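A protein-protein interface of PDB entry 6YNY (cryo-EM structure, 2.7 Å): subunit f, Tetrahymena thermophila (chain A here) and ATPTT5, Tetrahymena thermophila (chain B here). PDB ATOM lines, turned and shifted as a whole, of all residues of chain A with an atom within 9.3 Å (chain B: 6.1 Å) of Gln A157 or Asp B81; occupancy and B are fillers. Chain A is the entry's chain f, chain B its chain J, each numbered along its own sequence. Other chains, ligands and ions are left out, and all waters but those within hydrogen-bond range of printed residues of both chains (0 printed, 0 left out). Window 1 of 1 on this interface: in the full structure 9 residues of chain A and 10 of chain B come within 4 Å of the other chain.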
ATOM      1  N   TYR A 130      23.105   9.953  -7.894  1.00  0.00           N
ATOM      2  CA  TYR A 130      21.783   9.615  -7.383  1.00  0.00           C
ATOM      3  C   TYR A 130      21.608   8.109  -7.248  1.00  0.00           C
ATOM      4  O   TYR A 130      20.813   7.652  -6.422  1.00  0.00           O
ATOM      5  CB  TYR A 130      20.696  10.200  -8.284  1.00  0.00           C
ATOM      6  CG  TYR A 130      19.305  10.006  -7.742  1.00  0.00           C
ATOM      7  CD1 TYR A 130      18.755  10.910  -6.853  1.00  0.00           C
ATOM      8  CD2 TYR A 130      18.549   8.912  -8.111  1.00  0.00           C
ATOM      9  CE1 TYR A 130      17.490  10.731  -6.352  1.00  0.00           C
ATOM     10  CE2 TYR A 130      17.285   8.724  -7.615  1.00  0.00           C
ATOM     11  CZ  TYR A 130      16.760   9.635  -6.731  1.00  0.00           C
ATOM     12  OH  TYR A 130      15.493   9.458  -6.232  1.00  0.00           O
ATOM     13  N   GLY A 148      15.467   5.714 -10.943  1.00  0.00           N
ATOM     14  CA  GLY A 148      15.490   7.111 -11.310  1.00  0.00           C
ATOM     15  C   GLY A 148      14.743   7.981 -10.320  1.00  0.00           C
ATOM     16  O   GLY A 148      14.244   7.535  -9.287  1.00  0.00           O
ATOM     17  N   GLN A 149      14.669   9.265 -10.661  1.00  0.00           N
ATOM     18  CA  GLN A 149      13.981  10.255  -9.845  1.00  0.00           C
ATOM     19  C   GLN A 149      12.825  10.917 -10.580  1.00  0.00           C
ATOM     20  O   GLN A 149      12.318  11.945 -10.120  1.00  0.00           O
ATOM     21  CB  GLN A 149      14.967  11.319  -9.361  1.00  0.00           C
ATOM     22  CG  GLN A 149      15.974  11.749 -10.397  1.00  0.00           C
ATOM     23  CD  GLN A 149      16.941  12.775  -9.870  1.00  0.00           C
ATOM     24  OE1 GLN A 149      16.564  13.678  -9.126  1.00  0.00           O
ATOM     25  NE2 GLN A 149      18.202  12.639 -10.245  1.00  0.00           N
ATOM     26  N   VAL A 150      12.398  10.359 -11.707  1.00  0.00           N
ATOM     27  CA  VAL A 150      11.231  10.882 -12.431  1.00  0.00           C
ATOM     28  C   VAL A 150      10.024  10.169 -11.838  1.00  0.00           C
ATOM     29  O   VAL A 150       9.511   9.178 -12.364  1.00  0.00           O
ATOM     30  CB  VAL A 150      11.361  10.691 -13.942  1.00  0.00           C
ATOM     31  CG1 VAL A 150      10.182  11.293 -14.654  1.00  0.00           C
ATOM     32  CG2 VAL A 150      12.637  11.323 -14.424  1.00  0.00           C
ATOM     33  N   HIS A 151       9.548  10.701 -10.720  1.00  0.00           N
ATOM     34  CA  HIS A 151       8.506  10.045  -9.947  1.00  0.00           C
ATOM     35  C   HIS A 151       7.195  10.051 -10.719  1.00  0.00           C
ATOM     36  O   HIS A 151       6.633  11.113 -11.002  1.00  0.00           O
ATOM     37  CB  HIS A 151       8.348  10.736  -8.600  1.00  0.00           C
ATOM     38  CG  HIS A 151       9.626  10.852  -7.831  1.00  0.00           C
ATOM     39  ND1 HIS A 151      10.326   9.755  -7.384  1.00  0.00           N
ATOM     40  CD2 HIS A 151      10.329  11.935  -7.429  1.00  0.00           C
ATOM     41  CE1 HIS A 151      11.408  10.157  -6.742  1.00  0.00           C
ATOM     42  NE2 HIS A 151      11.433  11.475  -6.755  1.00  0.00           N
ATOM     43  N   PHE A 152       6.713   8.855 -11.054  1.00  0.00           N
ATOM     44  CA  PHE A 152       5.470   8.722 -11.801  1.00  0.00           C
ATOM     45  C   PHE A 152       4.265   9.147 -10.979  1.00  0.00           C
ATOM     46  O   PHE A 152       3.266   9.607 -11.541  1.00  0.00           O
ATOM     47  CB  PHE A 152       5.309   7.274 -12.259  1.00  0.00           C
ATOM     48  CG  PHE A 152       4.084   7.021 -13.080  1.00  0.00           C
ATOM     49  CD1 PHE A 152       4.120   7.136 -14.454  1.00  0.00           C
ATOM     50  CD2 PHE A 152       2.900   6.649 -12.480  1.00  0.00           C
ATOM     51  CE1 PHE A 152       2.997   6.896 -15.206  1.00  0.00           C
ATOM     52  CE2 PHE A 152       1.780   6.412 -13.227  1.00  0.00           C
ATOM     53  CZ  PHE A 152       1.827   6.533 -14.591  1.00  0.00           C
ATOM     54  N   GLY A 153       4.335   9.011  -9.665  1.00  0.00           N
ATOM     55  CA  GLY A 153       3.195   9.214  -8.794  1.00  0.00           C
ATOM     56  C   GLY A 153       3.148  10.594  -8.178  1.00  0.00           C
ATOM     57  O   GLY A 153       3.535  11.590  -8.798  1.00  0.00           O
ATOM     58  N   TYR A 154       2.673  10.648  -6.936  1.00  0.00           N
ATOM     59  CA  TYR A 154       2.404  11.909  -6.249  1.00  0.00           C
ATOM     60  C   TYR A 154       3.625  12.325  -5.433  1.00  0.00           C
ATOM     61  O   TYR A 154       3.657  12.265  -4.205  1.00  0.00           O
ATOM     62  CB  TYR A 154       1.169  11.775  -5.371  1.00  0.00           C
ATOM     63  CG  TYR A 154      -0.030  11.208  -6.085  1.00  0.00           C
ATOM     64  CD1 TYR A 154      -0.406  11.679  -7.330  1.00  0.00           C
ATOM     65  CD2 TYR A 154      -0.781  10.195  -5.516  1.00  0.00           C
ATOM     66  CE1 TYR A 154      -1.494  11.164  -7.981  1.00  0.00           C
ATOM     67  CE2 TYR A 154      -1.871   9.674  -6.162  1.00  0.00           C
ATOM     68  CZ  TYR A 154      -2.224  10.160  -7.394  1.00  0.00           C
ATOM     69  OH  TYR A 154      -3.316   9.637  -8.040  1.00  0.00           O
ATOM     70  N   HIS A 155       4.646  12.769  -6.158  1.00  0.00           N
ATOM     71  CA  HIS A 155       5.884  13.225  -5.556  1.00  0.00           C
ATOM     72  C   HIS A 155       6.416  14.406  -6.348  1.00  0.00           C
ATOM     73  O   HIS A 155       6.144  14.548  -7.543  1.00  0.00           O
ATOM     74  CB  HIS A 155       6.946  12.126  -5.518  1.00  0.00           C
ATOM     75  CG  HIS A 155       6.560  10.935  -4.705  1.00  0.00           C
ATOM     76  ND1 HIS A 155       6.631  10.920  -3.331  1.00  0.00           N
ATOM     77  CD2 HIS A 155       6.111   9.714  -5.073  1.00  0.00           C
ATOM     78  CE1 HIS A 155       6.237   9.741  -2.887  1.00  0.00           C
ATOM     79  NE2 HIS A 155       5.915   8.991  -3.923  1.00  0.00           N
ATOM     80  N   ASP A 156       7.171  15.252  -5.666  1.00  0.00           N
ATOM     81  CA  ASP A 156       7.864  16.345  -6.324  1.00  0.00           C
ATOM     82  C   ASP A 156       9.092  15.825  -7.054  1.00  0.00           C
ATOM     83  O   ASP A 156       9.839  14.994  -6.532  1.00  0.00           O
ATOM     84  CB  ASP A 156       8.282  17.406  -5.309  1.00  0.00           C
ATOM     85  CG  ASP A 156       7.103  18.119  -4.686  1.00  0.00           C
ATOM     86  OD1 ASP A 156       6.154  18.454  -5.421  1.00  0.00           O
ATOM     87  OD2 ASP A 156       7.127  18.349  -3.459  1.00  0.00           O
ATOM     88  N   GLN A 157       9.290  16.312  -8.269  1.00  0.00           N
ATOM     89  CA  GLN A 157      10.478  16.017  -9.051  1.00  0.00           C
ATOM     90  C   GLN A 157      11.442  17.188  -8.975  1.00  0.00           C
ATOM     91  O   GLN A 157      11.054  18.331  -8.723  1.00  0.00           O
ATOM     92  CB  GLN A 157      10.126  15.735 -10.510  1.00  0.00           C
ATOM     93  CG  GLN A 157       9.310  14.497 -10.728  1.00  0.00           C
ATOM     94  CD  GLN A 157       9.035  14.245 -12.188  1.00  0.00           C
ATOM     95  OE1 GLN A 157       9.643  14.859 -13.063  1.00  0.00           O
ATOM     96  NE2 GLN A 157       8.116  13.342 -12.462  1.00  0.00           N
ATOM     97  N   LYS A 158      12.720  16.889  -9.189  1.00  0.00           N
ATOM     98  CA  LYS A 158      13.770  17.902  -9.223  1.00  0.00           C
ATOM     99  C   LYS A 158      14.600  17.656 -10.474  1.00  0.00           C
ATOM    100  O   LYS A 158      15.570  16.896 -10.455  1.00  0.00           O
ATOM    101  CB  LYS A 158      14.620  17.865  -7.973  1.00  0.00           C
ATOM    102  CG  LYS A 158      15.507  19.072  -7.827  1.00  0.00           C
ATOM    103  CD  LYS A 158      16.397  18.967  -6.615  1.00  0.00           C
ATOM    104  CE  LYS A 158      17.177  20.247  -6.403  1.00  0.00           C
ATOM    105  NZ  LYS A 158      16.274  21.395  -6.153  1.00  0.00           N
ATOM    106  N   TRP A 159      14.206  18.301 -11.564  1.00  0.00           N
ATOM    107  CA  TRP A 159      14.952  18.197 -12.800  1.00  0.00           C
ATOM    108  C   TRP A 159      16.330  18.827 -12.632  1.00  0.00           C
ATOM    109  O   TRP A 159      16.567  19.643 -11.739  1.00  0.00           O
ATOM    110  CB  TRP A 159      14.202  18.880 -13.941  1.00  0.00           C
ATOM    111  CG  TRP A 159      12.963  18.179 -14.378  1.00  0.00           C
ATOM    112  CD1 TRP A 159      12.269  17.231 -13.693  1.00  0.00           C
ATOM    113  CD2 TRP A 159      12.264  18.374 -15.609  1.00  0.00           C
ATOM    114  NE1 TRP A 159      11.183  16.822 -14.419  1.00  0.00           N
ATOM    115  CE2 TRP A 159      11.157  17.510 -15.601  1.00  0.00           C
ATOM    116  CE3 TRP A 159      12.469  19.194 -16.719  1.00  0.00           C
ATOM    117  CZ2 TRP A 159      10.260  17.446 -16.653  1.00  0.00           C
ATOM    118  CZ3 TRP A 159      11.579  19.126 -17.760  1.00  0.00           C
ATOM    119  CH2 TRP A 159      10.488  18.259 -17.724  1.00  0.00           C
ATOM    120  N   GLY A 160      17.249  18.429 -13.503  1.00  0.00           N
ATOM    121  CA  GLY A 160      18.576  19.008 -13.467  1.00  0.00           C
ATOM    122  C   GLY A 160      18.544  20.494 -13.761  1.00  0.00           C
ATOM    123  O   GLY A 160      17.678  20.991 -14.482  1.00  0.00           O
ATOM    124  N   HIS B  79       0.072  20.318  -5.513  1.00  0.00           N
ATOM    125  CA  HIS B  79       0.746  20.355  -6.797  1.00  0.00           C
ATOM    126  C   HIS B  79       2.098  19.680  -6.644  1.00  0.00           C
ATOM    127  O   HIS B  79       2.551  19.393  -5.534  1.00  0.00           O
ATOM    128  CB  HIS B  79       0.904  21.788  -7.306  1.00  0.00           C
ATOM    129  CG  HIS B  79       1.814  22.629  -6.470  1.00  0.00           C
ATOM    130  ND1 HIS B  79       1.437  23.152  -5.253  1.00  0.00           N
ATOM    131  CD2 HIS B  79       3.085  23.044  -6.679  1.00  0.00           C
ATOM    132  CE1 HIS B  79       2.438  23.848  -4.746  1.00  0.00           C
ATOM    133  NE2 HIS B  79       3.449  23.800  -5.593  1.00  0.00           N
ATOM    134  N   PHE B  80       2.740  19.422  -7.777  1.00  0.00           N
ATOM    135  CA  PHE B  80       4.022  18.734  -7.795  1.00  0.00           C
ATOM    136  C   PHE B  80       4.956  19.447  -8.758  1.00  0.00           C
ATOM    137  O   PHE B  80       4.636  19.598  -9.941  1.00  0.00           O
ATOM    138  CB  PHE B  80       3.831  17.268  -8.178  1.00  0.00           C
ATOM    139  CG  PHE B  80       2.804  16.569  -7.343  1.00  0.00           C
ATOM    140  CD1 PHE B  80       3.103  16.168  -6.059  1.00  0.00           C
ATOM    141  CD2 PHE B  80       1.533  16.334  -7.829  1.00  0.00           C
ATOM    142  CE1 PHE B  80       2.169  15.543  -5.286  1.00  0.00           C
ATOM    143  CE2 PHE B  80       0.596  15.705  -7.054  1.00  0.00           C
ATOM    144  CZ  PHE B  80       0.915  15.309  -5.782  1.00  0.00           C
ATOM    145  N   ASP B  81       6.102  19.882  -8.246  1.00  0.00           N
ATOM    146  CA  ASP B  81       7.056  20.666  -9.011  1.00  0.00           C
ATOM    147  C   ASP B  81       8.027  19.764  -9.759  1.00  0.00           C
ATOM    148  O   ASP B  81       8.274  18.622  -9.364  1.00  0.00           O
ATOM    149  CB  ASP B  81       7.836  21.602  -8.092  1.00  0.00           C
ATOM    150  CG  ASP B  81       6.938  22.521  -7.295  1.00  0.00           C
ATOM    151  OD1 ASP B  81       6.465  22.105  -6.217  1.00  0.00           O
ATOM    152  OD2 ASP B  81       6.697  23.660  -7.746  1.00  0.00           O
ATOM    153  N   ARG B  82       8.572  20.289 -10.855  1.00  0.00           N
ATOM    154  CA  ARG B  82       9.516  19.552 -11.682  1.00  0.00           C
ATOM    155  C   ARG B  82      10.883  20.214 -11.741  1.00  0.00           C
ATOM    156  O   ARG B  82      11.892  19.570 -11.437  1.00  0.00           O
ATOM    157  CB  ARG B  82       8.953  19.390 -13.098  1.00  0.00           C
ATOM    158  CG  ARG B  82       7.452  19.150 -13.153  1.00  0.00           C
ATOM    159  CD  ARG B  82       7.012  18.027 -12.256  1.00  0.00           C
ATOM    160  NE  ARG B  82       6.155  17.085 -12.950  1.00  0.00           N
ATOM    161  CZ  ARG B  82       5.631  16.012 -12.377  1.00  0.00           C
ATOM    162  NH1 ARG B  82       5.869  15.757 -11.101  1.00  0.00           N
ATOM    163  NH2 ARG B  82       4.867  15.197 -13.081  1.00  0.00           N
ATOM    164  N   VAL B  83      10.945  21.488 -12.109  1.00  0.00           N
ATOM    165  CA  VAL B  83      12.209  22.204 -12.270  1.00  0.00           C
ATOM    166  C   VAL B  83      12.499  23.095 -11.074  1.00  0.00           C
ATOM    167  O   VAL B  83      13.597  23.063 -10.519  1.00  0.00           O
ATOM    168  CB  VAL B  83      12.206  23.017 -13.582  1.00  0.00           C
ATOM    169  CG1 VAL B  83      13.429  23.892 -13.666  1.00  0.00           C
ATOM    170  CG2 VAL B  83      12.168  22.095 -14.762  1.00  0.00           C
ATOM    171  N   PHE B  84      11.529  23.901 -10.663  1.00  0.00           N
ATOM    172  CA  PHE B  84      11.719  24.829  -9.561  1.00  0.00           C
ATOM    173  C   PHE B  84      10.404  24.966  -8.814  1.00  0.00           C
ATOM    174  O   PHE B  84       9.337  24.682  -9.370  1.00  0.00           O
ATOM    175  CB  PHE B  84      12.205  26.197 -10.057  1.00  0.00           C
ATOM    176  CG  PHE B  84      11.227  26.911 -10.938  1.00  0.00           C
ATOM    177  CD1 PHE B  84      10.248  27.721 -10.397  1.00  0.00           C
ATOM    178  CD2 PHE B  84      11.301  26.789 -12.311  1.00  0.00           C
ATOM    179  CE1 PHE B  84       9.354  28.380 -11.206  1.00  0.00           C
ATOM    180  CE2 PHE B  84      10.411  27.448 -13.123  1.00  0.00           C
ATOM    181  CZ  PHE B  84       9.436  28.246 -12.570  1.00  0.00           C
ATOM    182  N   PRO B  85      10.448  25.381  -7.549  1.00  0.00           N
ATOM    183  CA  PRO B  85       9.211  25.575  -6.778  1.00  0.00           C
ATOM    184  C   PRO B  85       8.420  26.772  -7.282  1.00  0.00           C
ATOM    185  O   PRO B  85       8.922  27.897  -7.309  1.00  0.00           O
ATOM    186  CB  PRO B  85       9.717  25.786  -5.349  1.00  0.00           C
ATOM    187  CG  PRO B  85      11.096  26.278  -5.507  1.00  0.00           C
ATOM    188  CD  PRO B  85      11.644  25.635  -6.735  1.00  0.00           C
ATOM    189  N   THR B  86       7.178  26.520  -7.679  1.00  0.00           N
ATOM    190  CA  THR B  86       6.333  27.548  -8.266  1.00  0.00           C
ATOM    191  C   THR B  86       5.504  28.294  -7.234  1.00  0.00           C
ATOM    192  O   THR B  86       5.075  29.421  -7.503  1.00  0.00           O
ATOM    193  CB  THR B  86       5.399  26.927  -9.302  1.00  0.00           C
ATOM    194  OG1 THR B  86       4.640  25.875  -8.694  1.00  0.00           O
ATOM    195  CG2 THR B  86       6.191  26.366 -10.454  1.00  0.00           C
ATOM    196  N   HIS B  87       5.271  27.696  -6.069  1.00  0.00           N
ATOM    197  CA  HIS B  87       4.407  28.274  -5.044  1.00  0.00           C
ATOM    198  C   HIS B  87       3.008  28.514  -5.601  1.00  0.00           C
ATOM    199  O   HIS B  87       2.458  29.614  -5.519  1.00  0.00           O
ATOM    200  CB  HIS B  87       5.007  29.562  -4.486  1.00  0.00           C
ATOM    201  CG  HIS B  87       6.374  29.388  -3.908  1.00  0.00           C
ATOM    202  ND1 HIS B  87       6.634  28.532  -2.861  1.00  0.00           N
ATOM    203  CD2 HIS B  87       7.558  29.958  -4.231  1.00  0.00           C
ATOM    204  CE1 HIS B  87       7.920  28.580  -2.566  1.00  0.00           C
ATOM    205  NE2 HIS B  87       8.502  29.439  -3.382  1.00  0.00           N
ATOM    206  N   TYR B  88       2.433  27.464  -6.176  1.00  0.00           N
ATOM    207  CA  TYR B  88       1.142  27.580  -6.834  1.00  0.00           C
ATOM    208  C   TYR B  88       0.059  27.949  -5.835  1.00  0.00           C
ATOM    209  O   TYR B  88      -0.093  27.304  -4.793  1.00  0.00           O
ATOM    210  CB  TYR B  88       0.797  26.271  -7.536  1.00  0.00           C
ATOM    211  CG  TYR B  88      -0.620  26.193  -8.036  1.00  0.00           C
ATOM    212  CD1 TYR B  88      -1.044  26.969  -9.100  1.00  0.00           C
ATOM    213  CD2 TYR B  88      -1.531  25.332  -7.455  1.00  0.00           C
ATOM    214  CE1 TYR B  88      -2.335  26.897  -9.560  1.00  0.00           C
ATOM    215  CE2 TYR B  88      -2.821  25.252  -7.911  1.00  0.00           C
ATOM    216  CZ  TYR B  88      -3.218  26.035  -8.963  1.00  0.00           C
ATOM    217  OH  TYR B  88      -4.509  25.958  -9.420  1.00  0.00           O
ATOM    218  N   LEU B 101       4.837  20.569 -18.675  1.00  0.00           N
ATOM    219  CA  LEU B 101       5.560  19.390 -18.211  1.00  0.00           C
ATOM    220  C   LEU B 101       6.734  19.763 -17.319  1.00  0.00           C
ATOM    221  O   LEU B 101       7.016  19.072 -16.336  1.00  0.00           O
ATOM    222  CB  LEU B 101       6.045  18.566 -19.402  1.00  0.00           C
ATOM    223  CG  LEU B 101       5.013  17.664 -20.071  1.00  0.00           C
ATOM    224  CD1 LEU B 101       5.544  17.147 -21.382  1.00  0.00           C
ATOM    225  CD2 LEU B 101       4.646  16.511 -19.163  1.00  0.00           C
ATOM    226  N   LEU B 103       7.087  22.481 -15.488  1.00  0.00           N
ATOM    227  CA  LEU B 103       6.734  23.439 -14.452  1.00  0.00           C
ATOM    228  C   LEU B 103       5.977  22.818 -13.290  1.00  0.00           C
ATOM    229  O   LEU B 103       6.371  23.002 -12.136  1.00  0.00           O
ATOM    230  CB  LEU B 103       5.906  24.579 -15.052  1.00  0.00           C
ATOM    231  CG  LEU B 103       6.607  25.472 -16.072  1.00  0.00           C
ATOM    232  CD1 LEU B 103       5.659  26.536 -16.567  1.00  0.00           C
ATOM    233  CD2 LEU B 103       7.847  26.104 -15.484  1.00  0.00           C
ATOM    234  N   ILE B 104       4.892  22.092 -13.553  1.00  0.00           N
ATOM    235  CA  ILE B 104       3.994  21.682 -12.485  1.00  0.00           C
ATOM    236  C   ILE B 104       3.178  20.484 -12.940  1.00  0.00           C
ATOM    237  O   ILE B 104       2.924  20.301 -14.132  1.00  0.00           O
ATOM    238  CB  ILE B 104       3.078  22.859 -12.066  1.00  0.00           C
ATOM    239  CG1 ILE B 104       2.464  22.605 -10.698  1.00  0.00           C
ATOM    240  CG2 ILE B 104       1.982  23.063 -13.077  1.00  0.00           C
ATOM    241  CD1 ILE B 104       1.616  23.729 -10.222  1.00  0.00           C
ATOM    242  N   LYS B 105       2.769  19.667 -11.975  1.00  0.00           N
ATOM    243  CA  LYS B 105       1.726  18.671 -12.155  1.00  0.00           C
ATOM    244  C   LYS B 105       0.691  18.881 -11.065  1.00  0.00           C
ATOM    245  O   LYS B 105       1.040  18.975  -9.885  1.00  0.00           O
ATOM    246  CB  LYS B 105       2.264  17.240 -12.087  1.00  0.00           C
ATOM    247  CG  LYS B 105       1.179  16.189 -12.208  1.00  0.00           C
ATOM    248  CD  LYS B 105       1.720  14.788 -12.306  1.00  0.00           C
ATOM    249  CE  LYS B 105       2.329  14.322 -11.007  1.00  0.00           C
ATOM    250  NZ  LYS B 105       2.883  12.956 -11.129  1.00  0.00           N
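Gln A157 touches just these residues of chain B: Asp B81 and Arg B82. Asp B81 touches just these residues of chain A: Asp A156 (3.2 Å) and Gln A157 (2.8 Å). Printed residues of chain A within 4 Å of Arg B82: His A155, Gln A157, Lys A158 and Trp A159. Of the printed residues of chain A, Leu B101 touches Trp A159. Of the printed residues of chain B, Asp A156 touches His B79 (3.7 Å), Phe B80 (3.2 Å) and Asp B81 (3.2 Å). Printed residues of chain A within 4 Å of Lys B105: Phe A152 and Gly A153. Printed residues of chain B within 4 Å of Gly A153: Lys B105 (2.8 Å). The nearest printed residue of chain B that does not touch Phe A152 is Arg B82 (6.0 Å).
N of Asp B81 sits at hydrogen-bond distance from OD1 of Asp A156 (3.2 Å). N of Gln A157 lies within hydrogen-bond range of O of Asp B81 (2.8 Å). The backbone carbonyl oxygen (O) of Arg B82 lies within hydrogen-bond range of the backbone NH (N) of Trp A159 (2.6 Å). NZ of Lys B105 is in hydrogen-bond range of O of Phe A152 (3.4 Å). The side-chain amino group of Lys B105 is in hydrogen-bond range of the backbone carbonyl oxygen of Gly A153, 2.8 Å away. O of Arg B82 lies close to O of Gln A157 (3.1 Å).
Among the printed residues, merely in contact across the chains: Tyr A154 with Phe B80 (3.5 Å), His A155 with Phe B80 (3.6 Å), His A155 with Arg B82 (3.8 Å), Asp A156 with His B79 (3.7 Å), Asp A156 with Phe B80 (3.2 Å), Lys A158 with Arg B82 (3.3 Å), Trp A159 with Val B83 (3.5 Å) and Trp A159 with Leu B101 (3.6 Å).
Hydrophobic or aromatic side chains of chain A that line the printed part of chain B: Tyr A154 and Trp A159. Along chain A the printed residues that touch a printed residue of chain B span positions 152 to 159. Printed residues of chain B that touch a printed residue of chain A: His B79, Phe B80, Asp B81, Arg B82, Val B83, Leu B101 and Lys B105. Hydrophobic or aromatic side chains of chain B within 4 Å of the printed part of chain A: Phe B80 and Val B83. Among the printed residues, 14 pairs touch across the chains. Among the printed residues, no Asp or Glu carboxylate lies within 4 Å of a Lys or Arg side-chain nitrogen of the other chain.
O of Lys B105 sits at hydrogen-bond distance from N of Phe B80. The side-chain carboxylate (OD2) of Asp B81 is in hydrogen-bond range of the backbone NH (N) of Thr B86, 2.9 Å away. The backbone carbonyl oxygen of His A151 sits at hydrogen-bond distance from the side-chain amide nitrogen of Gln A157 (3.0 Å). OE1 of Gln A157 lies within hydrogen-bond range of NE1 of Trp A159, at 2.8 Å.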
